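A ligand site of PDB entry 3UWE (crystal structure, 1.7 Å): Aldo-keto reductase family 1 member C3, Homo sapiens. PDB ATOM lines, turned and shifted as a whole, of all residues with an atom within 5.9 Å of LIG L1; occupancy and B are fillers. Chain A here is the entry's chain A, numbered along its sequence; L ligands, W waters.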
ATOM      1  N   TYR A  24       2.869  19.279  -8.658  1.00  0.00           N
ATOM      2  CA  TYR A  24       4.258  19.273  -9.097  1.00  0.00           C
ATOM      3  C   TYR A  24       4.385  20.024 -10.451  1.00  0.00           C
ATOM      4  O   TYR A  24       3.586  19.814 -11.352  1.00  0.00           O
ATOM      5  CB  TYR A  24       4.742  17.837  -9.348  1.00  0.00           C
ATOM      6  CG  TYR A  24       6.188  17.905  -9.841  1.00  0.00           C
ATOM      7  CD1 TYR A  24       7.230  18.273  -8.982  1.00  0.00           C
ATOM      8  CD2 TYR A  24       6.496  17.663 -11.183  1.00  0.00           C
ATOM      9  CE1 TYR A  24       8.571  18.371  -9.477  1.00  0.00           C
ATOM     10  CE2 TYR A  24       7.848  17.781 -11.681  1.00  0.00           C
ATOM     11  CZ  TYR A  24       8.851  18.104 -10.840  1.00  0.00           C
ATOM     12  OH  TYR A  24      10.153  18.227 -11.271  1.00  0.00           O
ATOM     13  N   ALA A  52       4.697  17.881  -1.654  1.00  0.00           N
ATOM     14  CA  ALA A  52       5.767  17.017  -1.194  1.00  0.00           C
ATOM     15  C   ALA A  52       7.023  17.846  -1.029  1.00  0.00           C
ATOM     16  O   ALA A  52       7.178  18.840  -1.727  1.00  0.00           O
ATOM     17  CB  ALA A  52       6.101  15.832  -2.283  1.00  0.00           C
ATOM     18  N   LEU A  54       9.851  17.008  -2.181  1.00  0.00           N
ATOM     19  CA  LEU A  54      10.511  16.926  -3.509  1.00  0.00           C
ATOM     20  C   LEU A  54      10.123  18.122  -4.416  1.00  0.00           C
ATOM     21  O   LEU A  54      10.933  18.559  -5.229  1.00  0.00           O
ATOM     22  CB  LEU A  54      10.125  15.603  -4.207  1.00  0.00           C
ATOM     23  CG  LEU A  54      10.821  15.317  -5.544  1.00  0.00           C
ATOM     24  CD1 LEU A  54      12.361  15.096  -5.384  1.00  0.00           C
ATOM     25  CD2 LEU A  54      10.176  14.136  -6.290  1.00  0.00           C
ATOM     26  N   TYR A  55       8.931  18.650  -4.254  1.00  0.00           N
ATOM     27  CA  TYR A  55       8.376  19.572  -5.270  1.00  0.00           C
ATOM     28  C   TYR A  55       8.904  21.007  -5.129  1.00  0.00           C
ATOM     29  O   TYR A  55       8.754  21.806  -6.106  1.00  0.00           O
ATOM     30  CB  TYR A  55       6.841  19.594  -5.192  1.00  0.00           C
ATOM     31  CG  TYR A  55       6.178  18.233  -5.404  1.00  0.00           C
ATOM     32  CD1 TYR A  55       6.940  17.163  -5.822  1.00  0.00           C
ATOM     33  CD2 TYR A  55       4.758  18.080  -5.171  1.00  0.00           C
ATOM     34  CE1 TYR A  55       6.353  15.889  -5.984  1.00  0.00           C
ATOM     35  CE2 TYR A  55       4.114  16.820  -5.323  1.00  0.00           C
ATOM     36  CZ  TYR A  55       4.883  15.740  -5.749  1.00  0.00           C
ATOM     37  OH  TYR A  55       4.347  14.482  -5.845  1.00  0.00           O
ATOM     38  N   LYS A  84       4.887  14.737   1.660  1.00  0.00           N
ATOM     39  CA  LYS A  84       5.522  13.394   1.505  1.00  0.00           C
ATOM     40  C   LYS A  84       6.943  13.469   1.995  1.00  0.00           C
ATOM     41  O   LYS A  84       7.643  14.494   1.726  1.00  0.00           O
ATOM     42  CB  LYS A  84       5.513  12.927   0.030  1.00  0.00           C
ATOM     43  CG  LYS A  84       4.111  13.007  -0.623  1.00  0.00           C
ATOM     44  CD  LYS A  84       4.211  12.302  -2.004  1.00  0.00           C
ATOM     45  CE  LYS A  84       2.871  12.588  -2.778  1.00  0.00           C
ATOM     46  NZ  LYS A  84       2.870  13.968  -3.383  1.00  0.00           N
ATOM     47  N   TRP A  86      10.645  12.679   1.701  1.00  0.00           N
ATOM     48  CA  TRP A  86      11.511  12.280   0.606  1.00  0.00           C
ATOM     49  C   TRP A  86      12.493  11.128   1.007  1.00  0.00           C
ATOM     50  O   TRP A  86      12.718  10.901   2.182  1.00  0.00           O
ATOM     51  CB  TRP A  86      12.237  13.565   0.074  1.00  0.00           C
ATOM     52  CG  TRP A  86      13.062  13.162  -1.171  1.00  0.00           C
ATOM     53  CD1 TRP A  86      14.399  13.246  -1.301  1.00  0.00           C
ATOM     54  CD2 TRP A  86      12.579  12.426  -2.338  1.00  0.00           C
ATOM     55  NE1 TRP A  86      14.811  12.691  -2.509  1.00  0.00           N
ATOM     56  CE2 TRP A  86      13.706  12.187  -3.164  1.00  0.00           C
ATOM     57  CE3 TRP A  86      11.310  12.015  -2.777  1.00  0.00           C
ATOM     58  CZ2 TRP A  86      13.618  11.529  -4.410  1.00  0.00           C
ATOM     59  CZ3 TRP A  86      11.201  11.316  -4.003  1.00  0.00           C
ATOM     60  CH2 TRP A  86      12.359  11.113  -4.820  1.00  0.00           C
ATOM     61  N   HIS A 117       7.286   8.855   0.348  1.00  0.00           N
ATOM     62  CA  HIS A 117       7.035   9.201  -1.065  1.00  0.00           C
ATOM     63  C   HIS A 117       7.371   7.957  -1.896  1.00  0.00           C
ATOM     64  O   HIS A 117       6.835   7.814  -2.994  1.00  0.00           O
ATOM     65  CB  HIS A 117       8.029  10.320  -1.458  1.00  0.00           C
ATOM     66  CG  HIS A 117       7.638  11.116  -2.673  1.00  0.00           C
ATOM     67  ND1 HIS A 117       7.843  12.485  -2.716  1.00  0.00           N
ATOM     68  CD2 HIS A 117       7.113  10.755  -3.879  1.00  0.00           C
ATOM     69  CE1 HIS A 117       7.494  12.931  -3.925  1.00  0.00           C
ATOM     70  NE2 HIS A 117       7.011  11.903  -4.637  1.00  0.00           N
ATOM     71  N   SER A 118       8.397   7.183  -1.472  1.00  0.00           N
ATOM     72  CA  SER A 118       8.880   6.118  -2.368  1.00  0.00           C
ATOM     73  C   SER A 118       9.593   5.104  -1.447  1.00  0.00           C
ATOM     74  O   SER A 118      10.191   5.514  -0.470  1.00  0.00           O
ATOM     75  CB  SER A 118       9.875   6.743  -3.327  1.00  0.00           C
ATOM     76  OG  SER A 118      10.713   5.779  -3.886  1.00  0.00           O
ATOM     77  N   MET A 120      12.231   3.559  -2.369  1.00  0.00           N
ATOM     78  CA  MET A 120      13.587   3.488  -2.900  1.00  0.00           C
ATOM     79  C   MET A 120      14.468   4.421  -2.125  1.00  0.00           C
ATOM     80  O   MET A 120      14.715   5.566  -2.525  1.00  0.00           O
ATOM     81  CB  MET A 120      13.635   3.802  -4.403  1.00  0.00           C
ATOM     82  CG  MET A 120      12.900   2.676  -5.195  1.00  0.00           C
ATOM     83  SD  MET A 120      12.881   3.054  -6.956  1.00  0.00           S
ATOM     84  CE  MET A 120      11.676   4.397  -6.941  1.00  0.00           C
ATOM     85  N   ASN A 167       4.066   4.646  -4.062  1.00  0.00           N
ATOM     86  CA  ASN A 167       4.952   3.845  -4.924  1.00  0.00           C
ATOM     87  C   ASN A 167       5.326   2.464  -4.267  1.00  0.00           C
ATOM     88  O   ASN A 167       6.339   1.880  -4.624  1.00  0.00           O
ATOM     89  CB  ASN A 167       6.201   4.667  -5.250  1.00  0.00           C
ATOM     90  CG  ASN A 167       5.896   5.808  -6.183  1.00  0.00           C
ATOM     91  OD1 ASN A 167       5.438   5.570  -7.299  1.00  0.00           O
ATOM     92  ND2 ASN A 167       6.182   7.041  -5.775  1.00  0.00           N
ATOM     93  N   GLN A 190      -0.292   5.734  -2.799  1.00  0.00           N
ATOM     94  CA  GLN A 190      -0.427   6.614  -3.979  1.00  0.00           C
ATOM     95  C   GLN A 190       0.540   6.093  -5.065  1.00  0.00           C
ATOM     96  O   GLN A 190       1.738   6.005  -4.848  1.00  0.00           O
ATOM     97  CB  GLN A 190       0.016   8.056  -3.573  1.00  0.00           C
ATOM     98  CG  GLN A 190      -0.163   9.034  -4.773  1.00  0.00           C
ATOM     99  CD  GLN A 190       0.261  10.464  -4.472  1.00  0.00           C
ATOM    100  OE1 GLN A 190       1.067  10.993  -5.222  1.00  0.00           O
ATOM    101  NE2 GLN A 190      -0.394  11.117  -3.503  1.00  0.00           N
ATOM    102  N   TYR A 216      -1.749   8.686  -9.289  1.00  0.00           N
ATOM    103  CA  TYR A 216      -1.000   9.830  -9.910  1.00  0.00           C
ATOM    104  C   TYR A 216      -0.736   9.510 -11.376  1.00  0.00           C
ATOM    105  O   TYR A 216      -0.806   8.333 -11.814  1.00  0.00           O
ATOM    106  CB  TYR A 216       0.312  10.140  -9.163  1.00  0.00           C
ATOM    107  CG  TYR A 216       1.468   9.182  -9.274  1.00  0.00           C
ATOM    108  CD1 TYR A 216       2.169   9.077 -10.471  1.00  0.00           C
ATOM    109  CD2 TYR A 216       1.958   8.493  -8.155  1.00  0.00           C
ATOM    110  CE1 TYR A 216       3.291   8.221 -10.571  1.00  0.00           C
ATOM    111  CE2 TYR A 216       3.121   7.712  -8.233  1.00  0.00           C
ATOM    112  CZ  TYR A 216       3.775   7.570  -9.426  1.00  0.00           C
ATOM    113  OH  TYR A 216       4.924   6.843  -9.519  1.00  0.00           O
ATOM    114  N   ARG A 226      13.235  13.702 -18.021  1.00  0.00           N
ATOM    115  CA  ARG A 226      14.165  13.126 -17.034  1.00  0.00           C
ATOM    116  C   ARG A 226      13.771  11.687 -16.750  1.00  0.00           C
ATOM    117  O   ARG A 226      14.598  10.886 -16.368  1.00  0.00           O
ATOM    118  CB  ARG A 226      14.160  13.924 -15.722  1.00  0.00           C
ATOM    119  CG  ARG A 226      14.893  15.349 -15.838  1.00  0.00           C
ATOM    120  CD  ARG A 226      14.733  16.223 -14.606  1.00  0.00           C
ATOM    121  NE  ARG A 226      13.372  16.775 -14.576  1.00  0.00           N
ATOM    122  CZ  ARG A 226      12.843  17.425 -13.528  1.00  0.00           C
ATOM    123  NH1 ARG A 226      13.598  17.609 -12.427  1.00  0.00           N
ATOM    124  NH2 ARG A 226      11.583  17.890 -13.585  1.00  0.00           N
ATOM    125  N   TRP A 227      12.481  11.332 -16.940  1.00  0.00           N
ATOM    126  CA  TRP A 227      12.051   9.965 -16.507  1.00  0.00           C
ATOM    127  C   TRP A 227      11.142   9.283 -17.516  1.00  0.00           C
ATOM    128  O   TRP A 227      10.872   8.103 -17.339  1.00  0.00           O
ATOM    129  CB  TRP A 227      11.292  10.038 -15.128  1.00  0.00           C
ATOM    130  CG  TRP A 227      12.051  10.767 -14.144  1.00  0.00           C
ATOM    131  CD1 TRP A 227      13.189  10.336 -13.500  1.00  0.00           C
ATOM    132  CD2 TRP A 227      11.772  12.070 -13.671  1.00  0.00           C
ATOM    133  NE1 TRP A 227      13.675  11.358 -12.688  1.00  0.00           N
ATOM    134  CE2 TRP A 227      12.814  12.420 -12.765  1.00  0.00           C
ATOM    135  CE3 TRP A 227      10.771  13.014 -13.961  1.00  0.00           C
ATOM    136  CZ2 TRP A 227      12.862  13.660 -12.125  1.00  0.00           C
ATOM    137  CZ3 TRP A 227      10.821  14.256 -13.336  1.00  0.00           C
ATOM    138  CH2 TRP A 227      11.876  14.559 -12.398  1.00  0.00           C
ATOM    139  N   PHE A 306       6.840   6.553 -15.802  1.00  0.00           N
ATOM    140  CA  PHE A 306       8.151   6.800 -15.107  1.00  0.00           C
ATOM    141  C   PHE A 306       8.940   5.567 -15.337  1.00  0.00           C
ATOM    142  O   PHE A 306       8.584   4.525 -14.813  1.00  0.00           O
ATOM    143  CB  PHE A 306       7.946   7.038 -13.603  1.00  0.00           C
ATOM    144  CG  PHE A 306       7.445   8.411 -13.327  1.00  0.00           C
ATOM    145  CD1 PHE A 306       8.306   9.462 -12.991  1.00  0.00           C
ATOM    146  CD2 PHE A 306       6.059   8.687 -13.468  1.00  0.00           C
ATOM    147  CE1 PHE A 306       7.829  10.775 -12.735  1.00  0.00           C
ATOM    148  CE2 PHE A 306       5.548   9.977 -13.241  1.00  0.00           C
ATOM    149  CZ  PHE A 306       6.388  11.021 -12.851  1.00  0.00           C
ATOM    150  N   PHE A 311      15.476   4.558 -11.253  1.00  0.00           N
ATOM    151  CA  PHE A 311      14.635   3.714 -10.415  1.00  0.00           C
ATOM    152  C   PHE A 311      14.907   2.243 -10.645  1.00  0.00           C
ATOM    153  O   PHE A 311      14.869   1.464  -9.695  1.00  0.00           O
ATOM    154  CB  PHE A 311      13.137   3.993 -10.713  1.00  0.00           C
ATOM    155  CG  PHE A 311      12.793   5.468 -10.734  1.00  0.00           C
ATOM    156  CD1 PHE A 311      13.067   6.281  -9.617  1.00  0.00           C
ATOM    157  CD2 PHE A 311      12.225   6.058 -11.892  1.00  0.00           C
ATOM    158  CE1 PHE A 311      12.768   7.640  -9.636  1.00  0.00           C
ATOM    159  CE2 PHE A 311      11.896   7.463 -11.929  1.00  0.00           C
ATOM    160  CZ  PHE A 311      12.151   8.261 -10.838  1.00  0.00           C
HETATM  161  O1  LIG L   1       5.336  14.226  -8.775  1.00  0.00           O
HETATM  162  O2  LIG L   1       6.000  13.013  -7.039  1.00  0.00           O
HETATM  163  C1  LIG L   1       8.745   7.046  -7.920  1.00  0.00           C
HETATM  164  C2  LIG L   1       8.204   7.694  -9.008  1.00  0.00           C
HETATM  165  C3  LIG L   1       9.704   7.699  -7.153  1.00  0.00           C
HETATM  166  C4  LIG L   1       9.104  13.967 -10.410  1.00  0.00           C
HETATM  167  C5  LIG L   1       8.750   8.964  -9.269  1.00  0.00           C
HETATM  168  C6  LIG L   1      10.273   8.960  -7.369  1.00  0.00           C
HETATM  169  C7  LIG L   1       9.832  12.803 -10.120  1.00  0.00           C
HETATM  170  C8  LIG L   1       7.837  14.167  -9.779  1.00  0.00           C
HETATM  171  C9  LIG L   1       8.150  12.079  -8.502  1.00  0.00           C
HETATM  172  O3  LIG L   1      10.138  10.814  -8.880  1.00  0.00           O
HETATM  173  C10 LIG L   1       6.215  13.486  -8.213  1.00  0.00           C
HETATM  174  C11 LIG L   1       9.719   9.620  -8.457  1.00  0.00           C
HETATM  175  C12 LIG L   1       9.367  11.874  -9.198  1.00  0.00           C
HETATM  176  C13 LIG L   1       7.402  13.193  -8.853  1.00  0.00           C
HETATM  177  P1  LG2 L   2      -1.168  14.416 -14.587  1.00  0.00           P
HETATM  178  O1  LG2 L   2      -2.222  14.651 -13.573  1.00  0.00           O
HETATM  179  O2  LG2 L   2      -1.087  13.070 -15.197  1.00  0.00           O
HETATM  180  O3  LG2 L   2      -1.318  15.535 -15.728  1.00  0.00           O
HETATM  181  C1  LG2 L   2      -0.533  15.350 -16.919  1.00  0.00           C
HETATM  182  C2  LG2 L   2      -0.744  16.673 -17.758  1.00  0.00           C
HETATM  183  O4  LG2 L   2      -2.210  16.678 -18.012  1.00  0.00           O
HETATM  184  C3  LG2 L   2      -0.477  17.927 -16.940  1.00  0.00           C
HETATM  185  O5  LG2 L   2       0.810  18.413 -17.214  1.00  0.00           O
HETATM  186  C4  LG2 L   2      -1.549  18.904 -17.542  1.00  0.00           C
HETATM  187  O6  LG2 L   2      -1.000  19.949 -18.402  1.00  0.00           O
HETATM  188  C5  LG2 L   2      -2.511  18.045 -18.353  1.00  0.00           C
HETATM  189  N1  LG2 L   2      -3.945  18.256 -18.171  1.00  0.00           N
HETATM  190  C6  LG2 L   2      -4.540  18.404 -16.985  1.00  0.00           C
HETATM  191  N2  LG2 L   2      -5.843  18.555 -17.155  1.00  0.00           N
HETATM  192  C7  LG2 L   2      -6.083  18.412 -18.491  1.00  0.00           C
HETATM  193  C8  LG2 L   2      -7.258  18.517 -19.242  1.00  0.00           C
HETATM  194  N3  LG2 L   2      -8.484  18.729 -18.654  1.00  0.00           N
HETATM  195  N4  LG2 L   2      -7.157  18.352 -20.569  1.00  0.00           N
HETATM  196  C9  LG2 L   2      -5.950  18.215 -21.177  1.00  0.00           C
HETATM  197  N5  LG2 L   2      -4.786  18.141 -20.488  1.00  0.00           N
HETATM  198  C10 LG2 L   2      -4.891  18.239 -19.120  1.00  0.00           C
HETATM  199  O7  LG2 L   2       0.229  14.817 -13.954  1.00  0.00           O
HETATM  200  P2  LG2 L   2       1.289  14.240 -12.902  1.00  0.00           P
HETATM  201  O8  LG2 L   2       2.029  15.417 -12.455  1.00  0.00           O
HETATM  202  O9  LG2 L   2       2.001  13.052 -13.450  1.00  0.00           O
HETATM  203  O10 LG2 L   2       0.368  13.631 -11.753  1.00  0.00           O
HETATM  204  C11 LG2 L   2      -0.462  14.507 -10.946  1.00  0.00           C
HETATM  205  C12 LG2 L   2       0.159  14.756  -9.528  1.00  0.00           C
HETATM  206  O11 LG2 L   2       0.342  13.438  -8.900  1.00  0.00           O
HETATM  207  C13 LG2 L   2       1.565  15.362  -9.520  1.00  0.00           C
HETATM  208  O12 LG2 L   2       1.426  16.792  -9.703  1.00  0.00           O
HETATM  209  C14 LG2 L   2       1.947  15.069  -8.070  1.00  0.00           C
HETATM  210  O13 LG2 L   2       1.072  15.865  -7.179  1.00  0.00           O
HETATM  211  C15 LG2 L   2       1.391  13.645  -7.926  1.00  0.00           C
HETATM  212  N6  LG2 L   2       2.493  12.704  -8.393  1.00  0.00           N
HETATM  213  C16 LG2 L   2       3.060  11.920  -7.422  1.00  0.00           C
HETATM  214  C17 LG2 L   2       4.031  10.995  -7.715  1.00  0.00           C
HETATM  215  C18 LG2 L   2       4.611  10.137  -6.601  1.00  0.00           C
HETATM  216  O14 LG2 L   2       5.736   9.656  -6.764  1.00  0.00           O
HETATM  217  N7  LG2 L   2       3.809   9.975  -5.461  1.00  0.00           N
HETATM  218  C19 LG2 L   2       4.572  10.811  -9.035  1.00  0.00           C
HETATM  219  C20 LG2 L   2       3.998  11.632 -10.046  1.00  0.00           C
HETATM  220  C21 LG2 L   2       2.919  12.467  -9.698  1.00  0.00           C
HETATM  221  P3  LG2 L   2      -1.341  21.517 -18.029  1.00  0.00           P
HETATM  222  O15 LG2 L   2      -0.726  22.188 -19.271  1.00  0.00           O
HETATM  223  O16 LG2 L   2      -2.873  21.561 -17.962  1.00  0.00           O
HETATM  224  O17 LG2 L   2      -0.699  21.808 -16.697  1.00  0.00           O
HETATM  225  O   HOH W   1       4.968  14.669 -11.504  1.00  0.00           O
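An oxygen (O2) of LIG L1 lies within hydrogen-bond range of the side-chain hydroxyl of Tyr 55 (2.5 Å).
A ring nitrogen (NE2) of His 117 sits at hydrogen-bond distance from an oxygen (O2) of LIG L1 (2.8 Å).
NE2 of His 117 lies within hydrogen-bond range of O14 of LG2 L2 (3.3 Å).
O14 of LG2 L2 is in hydrogen-bond range of ND2 of Asn 167, 2.8 Å away.
O12 of LG2 L2 lies within hydrogen-bond range of N of Tyr 24, 3.1 Å away.
A nitrogen (N7) of LG2 L2 sits at hydrogen-bond distance from the side-chain amide oxygen (OE1) of Gln 190.
OH of Tyr 55 sits at hydrogen-bond distance from NZ of Lys 84.
The side-chain amide nitrogen (ND2) of Asn 167 is in hydrogen-bond range of the backbone carbonyl oxygen (O) of His 117 (3.0 Å).
The side-chain amide oxygen (OD1) of Asn 167 lies within hydrogen-bond range of the side-chain hydroxyl (OH) of Tyr 216 (2.6 Å).
The backbone carbonyl oxygen (O) of Gln 190 is in hydrogen-bond range of the backbone NH (N) of Asn 167 (2.8 Å).
OH of Tyr 24 lies within hydrogen-bond range of NH2 of Arg 226 (2.7 Å).
The backbone NH of Met 120 sits at hydrogen-bond distance from the side-chain hydroxyl of Ser 118 (3.1 Å).
Residues that only touch LIG L1: Tyr 24, Leu 54, Trp 86, Ser 118, Met 120, Asn 167, Tyr 216, Trp 227, Phe 306 and Phe 311.
Hydrophobic or aromatic side chains within 4 Å of LIG L1: Tyr 24, Leu 54, Tyr 55, Trp 86, His 117, Met 120, Trp 227, Phe 306 and Phe 311.
12 residues have an atom within 4 Å of LIG L1: Tyr 24, Leu 54, Tyr 55, Trp 86, His 117, Ser 118, Met 120, Asn 167, Tyr 216, Trp 227, Phe 306 and Phe 311.
The nearest printed residue that does not touch LIG L1 is Lys 84 (4.9 Å).
Water W1 lies within hydrogen-bond range of O1 of LIG L1 and O8 of LG2 L2.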
